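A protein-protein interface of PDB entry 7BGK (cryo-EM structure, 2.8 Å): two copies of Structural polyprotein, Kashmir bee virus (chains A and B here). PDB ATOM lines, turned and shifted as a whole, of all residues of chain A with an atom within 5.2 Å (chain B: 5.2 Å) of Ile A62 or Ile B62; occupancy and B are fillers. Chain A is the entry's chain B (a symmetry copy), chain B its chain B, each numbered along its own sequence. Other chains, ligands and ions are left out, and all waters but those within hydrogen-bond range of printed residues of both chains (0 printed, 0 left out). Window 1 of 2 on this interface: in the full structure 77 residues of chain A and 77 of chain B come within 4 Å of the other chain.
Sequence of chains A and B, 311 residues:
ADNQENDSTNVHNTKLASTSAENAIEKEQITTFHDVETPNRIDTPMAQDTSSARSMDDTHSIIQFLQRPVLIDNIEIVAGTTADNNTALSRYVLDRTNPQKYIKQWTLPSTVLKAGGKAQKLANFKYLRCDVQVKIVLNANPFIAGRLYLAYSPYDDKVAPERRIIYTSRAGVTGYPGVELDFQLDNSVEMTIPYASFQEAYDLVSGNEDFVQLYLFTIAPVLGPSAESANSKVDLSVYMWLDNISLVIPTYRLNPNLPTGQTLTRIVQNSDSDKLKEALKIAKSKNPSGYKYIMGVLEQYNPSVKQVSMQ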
ATOM      1  N   HIS A  60       6.854  11.092   1.611  1.00  0.00           N
ATOM      2  CA  HIS A  60       6.536  11.957   0.493  1.00  0.00           C
ATOM      3  C   HIS A  60       7.492  11.709  -0.665  1.00  0.00           C
ATOM      4  O   HIS A  60       8.655  11.351  -0.475  1.00  0.00           O
ATOM      5  CB  HIS A  60       6.589  13.423   0.920  1.00  0.00           C
ATOM      6  CG  HIS A  60       5.648  13.758   2.035  1.00  0.00           C
ATOM      7  ND1 HIS A  60       4.365  13.262   2.097  1.00  0.00           N
ATOM      8  CD2 HIS A  60       5.802  14.539   3.129  1.00  0.00           C
ATOM      9  CE1 HIS A  60       3.769  13.721   3.182  1.00  0.00           C
ATOM     10  NE2 HIS A  60       4.618  14.500   3.826  1.00  0.00           N
ATOM     11  N   SER A  61       6.979  11.892  -1.875  1.00  0.00           N
ATOM     12  CA  SER A  61       7.767  11.732  -3.080  1.00  0.00           C
ATOM     13  C   SER A  61       8.362  13.074  -3.490  1.00  0.00           C
ATOM     14  O   SER A  61       8.192  14.092  -2.819  1.00  0.00           O
ATOM     15  CB  SER A  61       6.920  11.147  -4.207  1.00  0.00           C
ATOM     16  OG  SER A  61       5.752  11.908  -4.431  1.00  0.00           O
ATOM     17  N   ILE A  62       9.079  13.074  -4.610  1.00  0.00           N
ATOM     18  CA  ILE A  62       9.592  14.323  -5.151  1.00  0.00           C
ATOM     19  C   ILE A  62       8.453  15.146  -5.731  1.00  0.00           C
ATOM     20  O   ILE A  62       8.440  16.375  -5.620  1.00  0.00           O
ATOM     21  CB  ILE A  62      10.685  14.037  -6.197  1.00  0.00           C
ATOM     22  CG1 ILE A  62      11.938  13.498  -5.517  1.00  0.00           C
ATOM     23  CG2 ILE A  62      11.036  15.287  -6.963  1.00  0.00           C
ATOM     24  CD1 ILE A  62      12.888  12.840  -6.443  1.00  0.00           C
ATOM     25  N   ILE A  63       7.476  14.486  -6.348  1.00  0.00           N
ATOM     26  CA  ILE A  63       6.315  15.197  -6.869  1.00  0.00           C
ATOM     27  C   ILE A  63       5.556  15.869  -5.739  1.00  0.00           C
ATOM     28  O   ILE A  63       5.051  16.986  -5.888  1.00  0.00           O
ATOM     29  CB  ILE A  63       5.424  14.233  -7.672  1.00  0.00           C
ATOM     30  CG1 ILE A  63       6.137  13.817  -8.954  1.00  0.00           C
ATOM     31  CG2 ILE A  63       4.097  14.864  -8.003  1.00  0.00           C
ATOM     32  CD1 ILE A  63       5.478  12.691  -9.682  1.00  0.00           C
ATOM     33  N   GLN A  64       5.456  15.201  -4.591  1.00  0.00           N
ATOM     34  CA  GLN A  64       4.806  15.812  -3.438  1.00  0.00           C
ATOM     35  C   GLN A  64       5.633  16.961  -2.885  1.00  0.00           C
ATOM     36  O   GLN A  64       5.090  18.019  -2.549  1.00  0.00           O
ATOM     37  CB  GLN A  64       4.574  14.771  -2.354  1.00  0.00           C
ATOM     38  CG  GLN A  64       3.583  13.705  -2.707  1.00  0.00           C
ATOM     39  CD  GLN A  64       3.248  12.835  -1.527  1.00  0.00           C
ATOM     40  OE1 GLN A  64       3.289  13.279  -0.385  1.00  0.00           O
ATOM     41  NE2 GLN A  64       2.938  11.581  -1.792  1.00  0.00           N
ATOM     42  N   PHE A  65       6.943  16.766  -2.766  1.00  0.00           N
ATOM     43  CA  PHE A  65       7.812  17.822  -2.268  1.00  0.00           C
ATOM     44  C   PHE A  65       7.707  19.075  -3.123  1.00  0.00           C
ATOM     45  O   PHE A  65       7.652  20.191  -2.599  1.00  0.00           O
ATOM     46  CB  PHE A  65       9.250  17.317  -2.221  1.00  0.00           C
ATOM     47  CG  PHE A  65      10.169  18.178  -1.421  1.00  0.00           C
ATOM     48  CD1 PHE A  65      10.573  17.784  -0.169  1.00  0.00           C
ATOM     49  CD2 PHE A  65      10.634  19.373  -1.922  1.00  0.00           C
ATOM     50  CE1 PHE A  65      11.413  18.565   0.569  1.00  0.00           C
ATOM     51  CE2 PHE A  65      11.470  20.154  -1.188  1.00  0.00           C
ATOM     52  CZ  PHE A  65      11.863  19.751   0.059  1.00  0.00           C
ATOM     53  N   LEU A  66       7.682  18.912  -4.444  1.00  0.00           N
ATOM     54  CA  LEU A  66       7.584  20.049  -5.345  1.00  0.00           C
ATOM     55  C   LEU A  66       6.201  20.677  -5.350  1.00  0.00           C
ATOM     56  O   LEU A  66       6.043  21.778  -5.884  1.00  0.00           O
ATOM     57  CB  LEU A  66       7.958  19.624  -6.758  1.00  0.00           C
ATOM     58  CG  LEU A  66       9.344  19.011  -6.951  1.00  0.00           C
ATOM     59  CD1 LEU A  66       9.520  18.559  -8.375  1.00  0.00           C
ATOM     60  CD2 LEU A  66      10.429  19.967  -6.568  1.00  0.00           C
ATOM     61  N   GLN A  67       5.207  20.010  -4.781  1.00  0.00           N
ATOM     62  CA  GLN A  67       3.865  20.549  -4.651  1.00  0.00           C
ATOM     63  C   GLN A  67       3.678  21.341  -3.369  1.00  0.00           C
ATOM     64  O   GLN A  67       2.549  21.730  -3.055  1.00  0.00           O
ATOM     65  CB  GLN A  67       2.842  19.422  -4.705  1.00  0.00           C
ATOM     66  CG  GLN A  67       2.633  18.828  -6.065  1.00  0.00           C
ATOM     67  CD  GLN A  67       1.856  17.545  -6.019  1.00  0.00           C
ATOM     68  OE1 GLN A  67       1.471  17.074  -4.953  1.00  0.00           O
ATOM     69  NE2 GLN A  67       1.612  16.969  -7.180  1.00  0.00           N
ATOM     70  N   LYS A 121      15.932  18.610  -4.889  1.00  0.00           N
ATOM     71  CA  LYS A 121      15.214  17.438  -5.365  1.00  0.00           C
ATOM     72  C   LYS A 121      15.195  17.344  -6.879  1.00  0.00           C
ATOM     73  O   LYS A 121      15.126  16.238  -7.424  1.00  0.00           O
ATOM     74  CB  LYS A 121      13.781  17.453  -4.837  1.00  0.00           C
ATOM     75  CG  LYS A 121      13.600  16.765  -3.512  1.00  0.00           C
ATOM     76  CD  LYS A 121      14.367  17.461  -2.432  1.00  0.00           C
ATOM     77  CE  LYS A 121      14.254  16.747  -1.120  1.00  0.00           C
ATOM     78  NZ  LYS A 121      14.817  17.563  -0.039  1.00  0.00           N
ATOM     79  N   PHE A 125      18.557  15.405 -12.366  1.00  0.00           N
ATOM     80  CA  PHE A 125      17.500  15.153 -13.327  1.00  0.00           C
ATOM     81  C   PHE A 125      17.640  16.142 -14.470  1.00  0.00           C
ATOM     82  O   PHE A 125      18.023  17.297 -14.260  1.00  0.00           O
ATOM     83  CB  PHE A 125      16.139  15.297 -12.705  1.00  0.00           C
ATOM     84  CG  PHE A 125      15.714  14.128 -11.870  1.00  0.00           C
ATOM     85  CD1 PHE A 125      15.424  12.911 -12.447  1.00  0.00           C
ATOM     86  CD2 PHE A 125      15.572  14.260 -10.504  1.00  0.00           C
ATOM     87  CE1 PHE A 125      15.023  11.854 -11.679  1.00  0.00           C
ATOM     88  CE2 PHE A 125      15.173  13.208  -9.737  1.00  0.00           C
ATOM     89  CZ  PHE A 125      14.895  12.004 -10.319  1.00  0.00           C
ATOM     90  N   LEU A 247       9.635  14.332 -13.633  1.00  0.00           N
ATOM     91  CA  LEU A 247      11.084  14.192 -13.680  1.00  0.00           C
ATOM     92  C   LEU A 247      11.410  12.783 -14.149  1.00  0.00           C
ATOM     93  O   LEU A 247      10.944  11.805 -13.558  1.00  0.00           O
ATOM     94  CB  LEU A 247      11.691  14.438 -12.300  1.00  0.00           C
ATOM     95  CG  LEU A 247      11.656  15.771 -11.550  1.00  0.00           C
ATOM     96  CD1 LEU A 247      12.234  15.668 -10.093  1.00  0.00           C
ATOM     97  CD2 LEU A 247      12.409  16.803 -12.278  1.00  0.00           C
ATOM     98  N   HIS B  60      10.738   9.094 -10.799  1.00  0.00           N
ATOM     99  CA  HIS B  60      11.254   8.387  -9.645  1.00  0.00           C
ATOM    100  C   HIS B  60      10.950   9.154  -8.367  1.00  0.00           C
ATOM    101  O   HIS B  60      10.879  10.385  -8.355  1.00  0.00           O
ATOM    102  CB  HIS B  60      12.759   8.163  -9.785  1.00  0.00           C
ATOM    103  CG  HIS B  60      13.139   7.381 -11.004  1.00  0.00           C
ATOM    104  ND1 HIS B  60      12.427   6.285 -11.434  1.00  0.00           N
ATOM    105  CD2 HIS B  60      14.158   7.534 -11.881  1.00  0.00           C
ATOM    106  CE1 HIS B  60      12.987   5.798 -12.525  1.00  0.00           C
ATOM    107  NE2 HIS B  60      14.041   6.537 -12.818  1.00  0.00           N
ATOM    108  N   SER B  61      10.756   8.408  -7.287  1.00  0.00           N
ATOM    109  CA  SER B  61      10.493   8.986  -5.985  1.00  0.00           C
ATOM    110  C   SER B  61      11.801   9.162  -5.225  1.00  0.00           C
ATOM    111  O   SER B  61      12.889   8.876  -5.727  1.00  0.00           O
ATOM    112  CB  SER B  61       9.518   8.118  -5.195  1.00  0.00           C
ATOM    113  OG  SER B  61       9.965   6.782  -5.104  1.00  0.00           O
ATOM    114  N   ILE B  62      11.695   9.650  -3.992  1.00  0.00           N
ATOM    115  CA  ILE B  62      12.870   9.747  -3.139  1.00  0.00           C
ATOM    116  C   ILE B  62      13.303   8.361  -2.689  1.00  0.00           C
ATOM    117  O   ILE B  62      14.499   8.075  -2.582  1.00  0.00           O
ATOM    118  CB  ILE B  62      12.582  10.675  -1.945  1.00  0.00           C
ATOM    119  CG1 ILE B  62      12.465  12.120  -2.415  1.00  0.00           C
ATOM    120  CG2 ILE B  62      13.675  10.577  -0.912  1.00  0.00           C
ATOM    121  CD1 ILE B  62      11.820  13.020  -1.433  1.00  0.00           C
ATOM    122  N   ILE B  63      12.343   7.476  -2.430  1.00  0.00           N
ATOM    123  CA  ILE B  63      12.679   6.107  -2.060  1.00  0.00           C
ATOM    124  C   ILE B  63      13.420   5.420  -3.195  1.00  0.00           C
ATOM    125  O   ILE B  63      14.355   4.646  -2.966  1.00  0.00           O
ATOM    126  CB  ILE B  63      11.404   5.344  -1.658  1.00  0.00           C
ATOM    127  CG1 ILE B  63      10.864   5.898  -0.344  1.00  0.00           C
ATOM    128  CG2 ILE B  63      11.672   3.867  -1.522  1.00  0.00           C
ATOM    129  CD1 ILE B  63       9.498   5.408   0.010  1.00  0.00           C
ATOM    130  N   GLN B  64      13.017   5.686  -4.436  1.00  0.00           N
ATOM    131  CA  GLN B  64      13.726   5.123  -5.577  1.00  0.00           C
ATOM    132  C   GLN B  64      15.109   5.736  -5.723  1.00  0.00           C
ATOM    133  O   GLN B  64      16.086   5.025  -5.979  1.00  0.00           O
ATOM    134  CB  GLN B  64      12.925   5.341  -6.851  1.00  0.00           C
ATOM    135  CG  GLN B  64      11.634   4.586  -6.921  1.00  0.00           C
ATOM    136  CD  GLN B  64      10.996   4.681  -8.279  1.00  0.00           C
ATOM    137  OE1 GLN B  64      11.682   4.816  -9.288  1.00  0.00           O
ATOM    138  NE2 GLN B  64       9.680   4.637  -8.315  1.00  0.00           N
ATOM    139  N   PHE B  65      15.208   7.055  -5.582  1.00  0.00           N
ATOM    140  CA  PHE B  65      16.498   7.721  -5.682  1.00  0.00           C
ATOM    141  C   PHE B  65      17.484   7.172  -4.663  1.00  0.00           C
ATOM    142  O   PHE B  65      18.656   6.947  -4.982  1.00  0.00           O
ATOM    143  CB  PHE B  65      16.309   9.224  -5.497  1.00  0.00           C
ATOM    144  CG  PHE B  65      17.489  10.037  -5.910  1.00  0.00           C
ATOM    145  CD1 PHE B  65      17.470  10.738  -7.092  1.00  0.00           C
ATOM    146  CD2 PHE B  65      18.613  10.108  -5.116  1.00  0.00           C
ATOM    147  CE1 PHE B  65      18.545  11.484  -7.475  1.00  0.00           C
ATOM    148  CE2 PHE B  65      19.686  10.850  -5.498  1.00  0.00           C
ATOM    149  CZ  PHE B  65      19.654  11.542  -6.679  1.00  0.00           C
ATOM    150  N   LEU B  66      17.032   6.954  -3.431  1.00  0.00           N
ATOM    151  CA  LEU B  66      17.900   6.431  -2.388  1.00  0.00           C
ATOM    152  C   LEU B  66      18.225   4.960  -2.578  1.00  0.00           C
ATOM    153  O   LEU B  66      19.127   4.453  -1.906  1.00  0.00           O
ATOM    154  CB  LEU B  66      17.255   6.641  -1.025  1.00  0.00           C
ATOM    155  CG  LEU B  66      16.901   8.076  -0.642  1.00  0.00           C
ATOM    156  CD1 LEU B  66      16.190   8.101   0.684  1.00  0.00           C
ATOM    157  CD2 LEU B  66      18.114   8.952  -0.600  1.00  0.00           C
ATOM    158  N   GLN B  67      17.518   4.270  -3.461  1.00  0.00           N
ATOM    159  CA  GLN B  67      17.796   2.883  -3.787  1.00  0.00           C
ATOM    160  C   GLN B  67      18.799   2.740  -4.919  1.00  0.00           C
ATOM    161  O   GLN B  67      19.018   1.626  -5.400  1.00  0.00           O
ATOM    162  CB  GLN B  67      16.506   2.164  -4.160  1.00  0.00           C
ATOM    163  CG  GLN B  67      15.598   1.867  -3.005  1.00  0.00           C
ATOM    164  CD  GLN B  67      14.228   1.438  -3.448  1.00  0.00           C
ATOM    165  OE1 GLN B  67      13.938   1.370  -4.638  1.00  0.00           O
ATOM    166  NE2 GLN B  67      13.373   1.138  -2.490  1.00  0.00           N
ATOM    167  N   LYS B 121      18.276  14.827  -1.235  1.00  0.00           N
ATOM    168  CA  LYS B 121      16.908  14.337  -1.143  1.00  0.00           C
ATOM    169  C   LYS B 121      16.480  14.075   0.289  1.00  0.00           C
ATOM    170  O   LYS B 121      15.290  14.176   0.601  1.00  0.00           O
ATOM    171  CB  LYS B 121      16.757  13.057  -1.963  1.00  0.00           C
ATOM    172  CG  LYS B 121      16.357  13.283  -3.395  1.00  0.00           C
ATOM    173  CD  LYS B 121      17.412  14.039  -4.139  1.00  0.00           C
ATOM    174  CE  LYS B 121      16.997  14.332  -5.549  1.00  0.00           C
ATOM    175  NZ  LYS B 121      18.126  14.866  -6.318  1.00  0.00           N
ATOM    176  N   PHE B 125      14.080  16.780   5.953  1.00  0.00           N
ATOM    177  CA  PHE B 125      13.419  15.661   6.598  1.00  0.00           C
ATOM    178  C   PHE B 125      14.138  15.358   7.899  1.00  0.00           C
ATOM    179  O   PHE B 125      15.363  15.486   7.985  1.00  0.00           O
ATOM    180  CB  PHE B 125      13.424  14.437   5.725  1.00  0.00           C
ATOM    181  CG  PHE B 125      12.409  14.456   4.624  1.00  0.00           C
ATOM    182  CD1 PHE B 125      11.061  14.368   4.898  1.00  0.00           C
ATOM    183  CD2 PHE B 125      12.809  14.530   3.306  1.00  0.00           C
ATOM    184  CE1 PHE B 125      10.143  14.372   3.887  1.00  0.00           C
ATOM    185  CE2 PHE B 125      11.895  14.534   2.297  1.00  0.00           C
ATOM    186  CZ  PHE B 125      10.561  14.453   2.580  1.00  0.00           C
ATOM    187  N   LEU B 247      11.013   8.291   5.008  1.00  0.00           N
ATOM    188  CA  LEU B 247      11.155   9.701   5.349  1.00  0.00           C
ATOM    189  C   LEU B 247       9.771  10.265   5.623  1.00  0.00           C
ATOM    190  O   LEU B 247       8.876  10.157   4.780  1.00  0.00           O
ATOM    191  CB  LEU B 247      11.816  10.465   4.203  1.00  0.00           C
ATOM    192  CG  LEU B 247      13.247  10.246   3.710  1.00  0.00           C
ATOM    193  CD1 LEU B 247      13.585  11.079   2.422  1.00  0.00           C
ATOM    194  CD2 LEU B 247      14.220  10.590   4.757  1.00  0.00           C
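The side-chain amino group of Lys A121 sits close to the backbone carbonyl oxygen of Lys B121 (3.5 Å).
A ring nitrogen (ND1) of His B60 is in hydrogen-bond range of the side-chain amide oxygen of Gln B64, at 2.7 Å. The side-chain amide oxygen (OE1) of Gln A64 sits at hydrogen-bond distance from a ring nitrogen (ND1) of His A60.
Among the printed residues, merely in contact across the chains: Ile A62 with Ile B62, Ile A62 with His B60, His A60 with Ile B62, Leu A247 with His B60 and His A60 with Leu B247.
Printed residues of chain B within 4 Å of His A60: Ile B62 and Leu B247. Of chain B, only His B60 (3.7 Å) and Ile B62 (3.4 Å) come within 4 Å of Ile A62. Of the printed residues of chain B, Lys A121 touches Lys B121. Of the printed residues of chain B, Leu A247 touches His B60 (3.9 Å). Of chain A, only His A60 (3.7 Å) and Ile A62 (3.4 Å) come within 4 Å of Ile B62. Of the printed residues of chain A, Lys B121 touches Lys A121. The nearest residue of chain A that does not touch Ile B62 is Ser A61 (4.02 Å).
Of the 11 printed residues of chain A, 4 touch a printed residue of chain B. Printed residues of chain A that touch a printed residue of chain B: His A60, Ile A62, Lys A121 and Leu A247. Of the 11 printed residues of chain B, 4 touch a printed residue of chain A. Among the printed residues, 6 pairs touch across the chains. Among the printed residues, no Asp or Glu carboxylate lies within 4 Å of a Lys or Arg side-chain nitrogen of the other chain.
His A60 touches Ile B62, and with the chains exchanged Ile A62 touches His B60. His A60 touches Leu B247, and with the chains exchanged Leu A247 touches His B60. Ile B62 touches its own counterpart, Ile A62. Lys A121 touches its own counterpart, Lys B121. 11 positions are printed for both chains.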
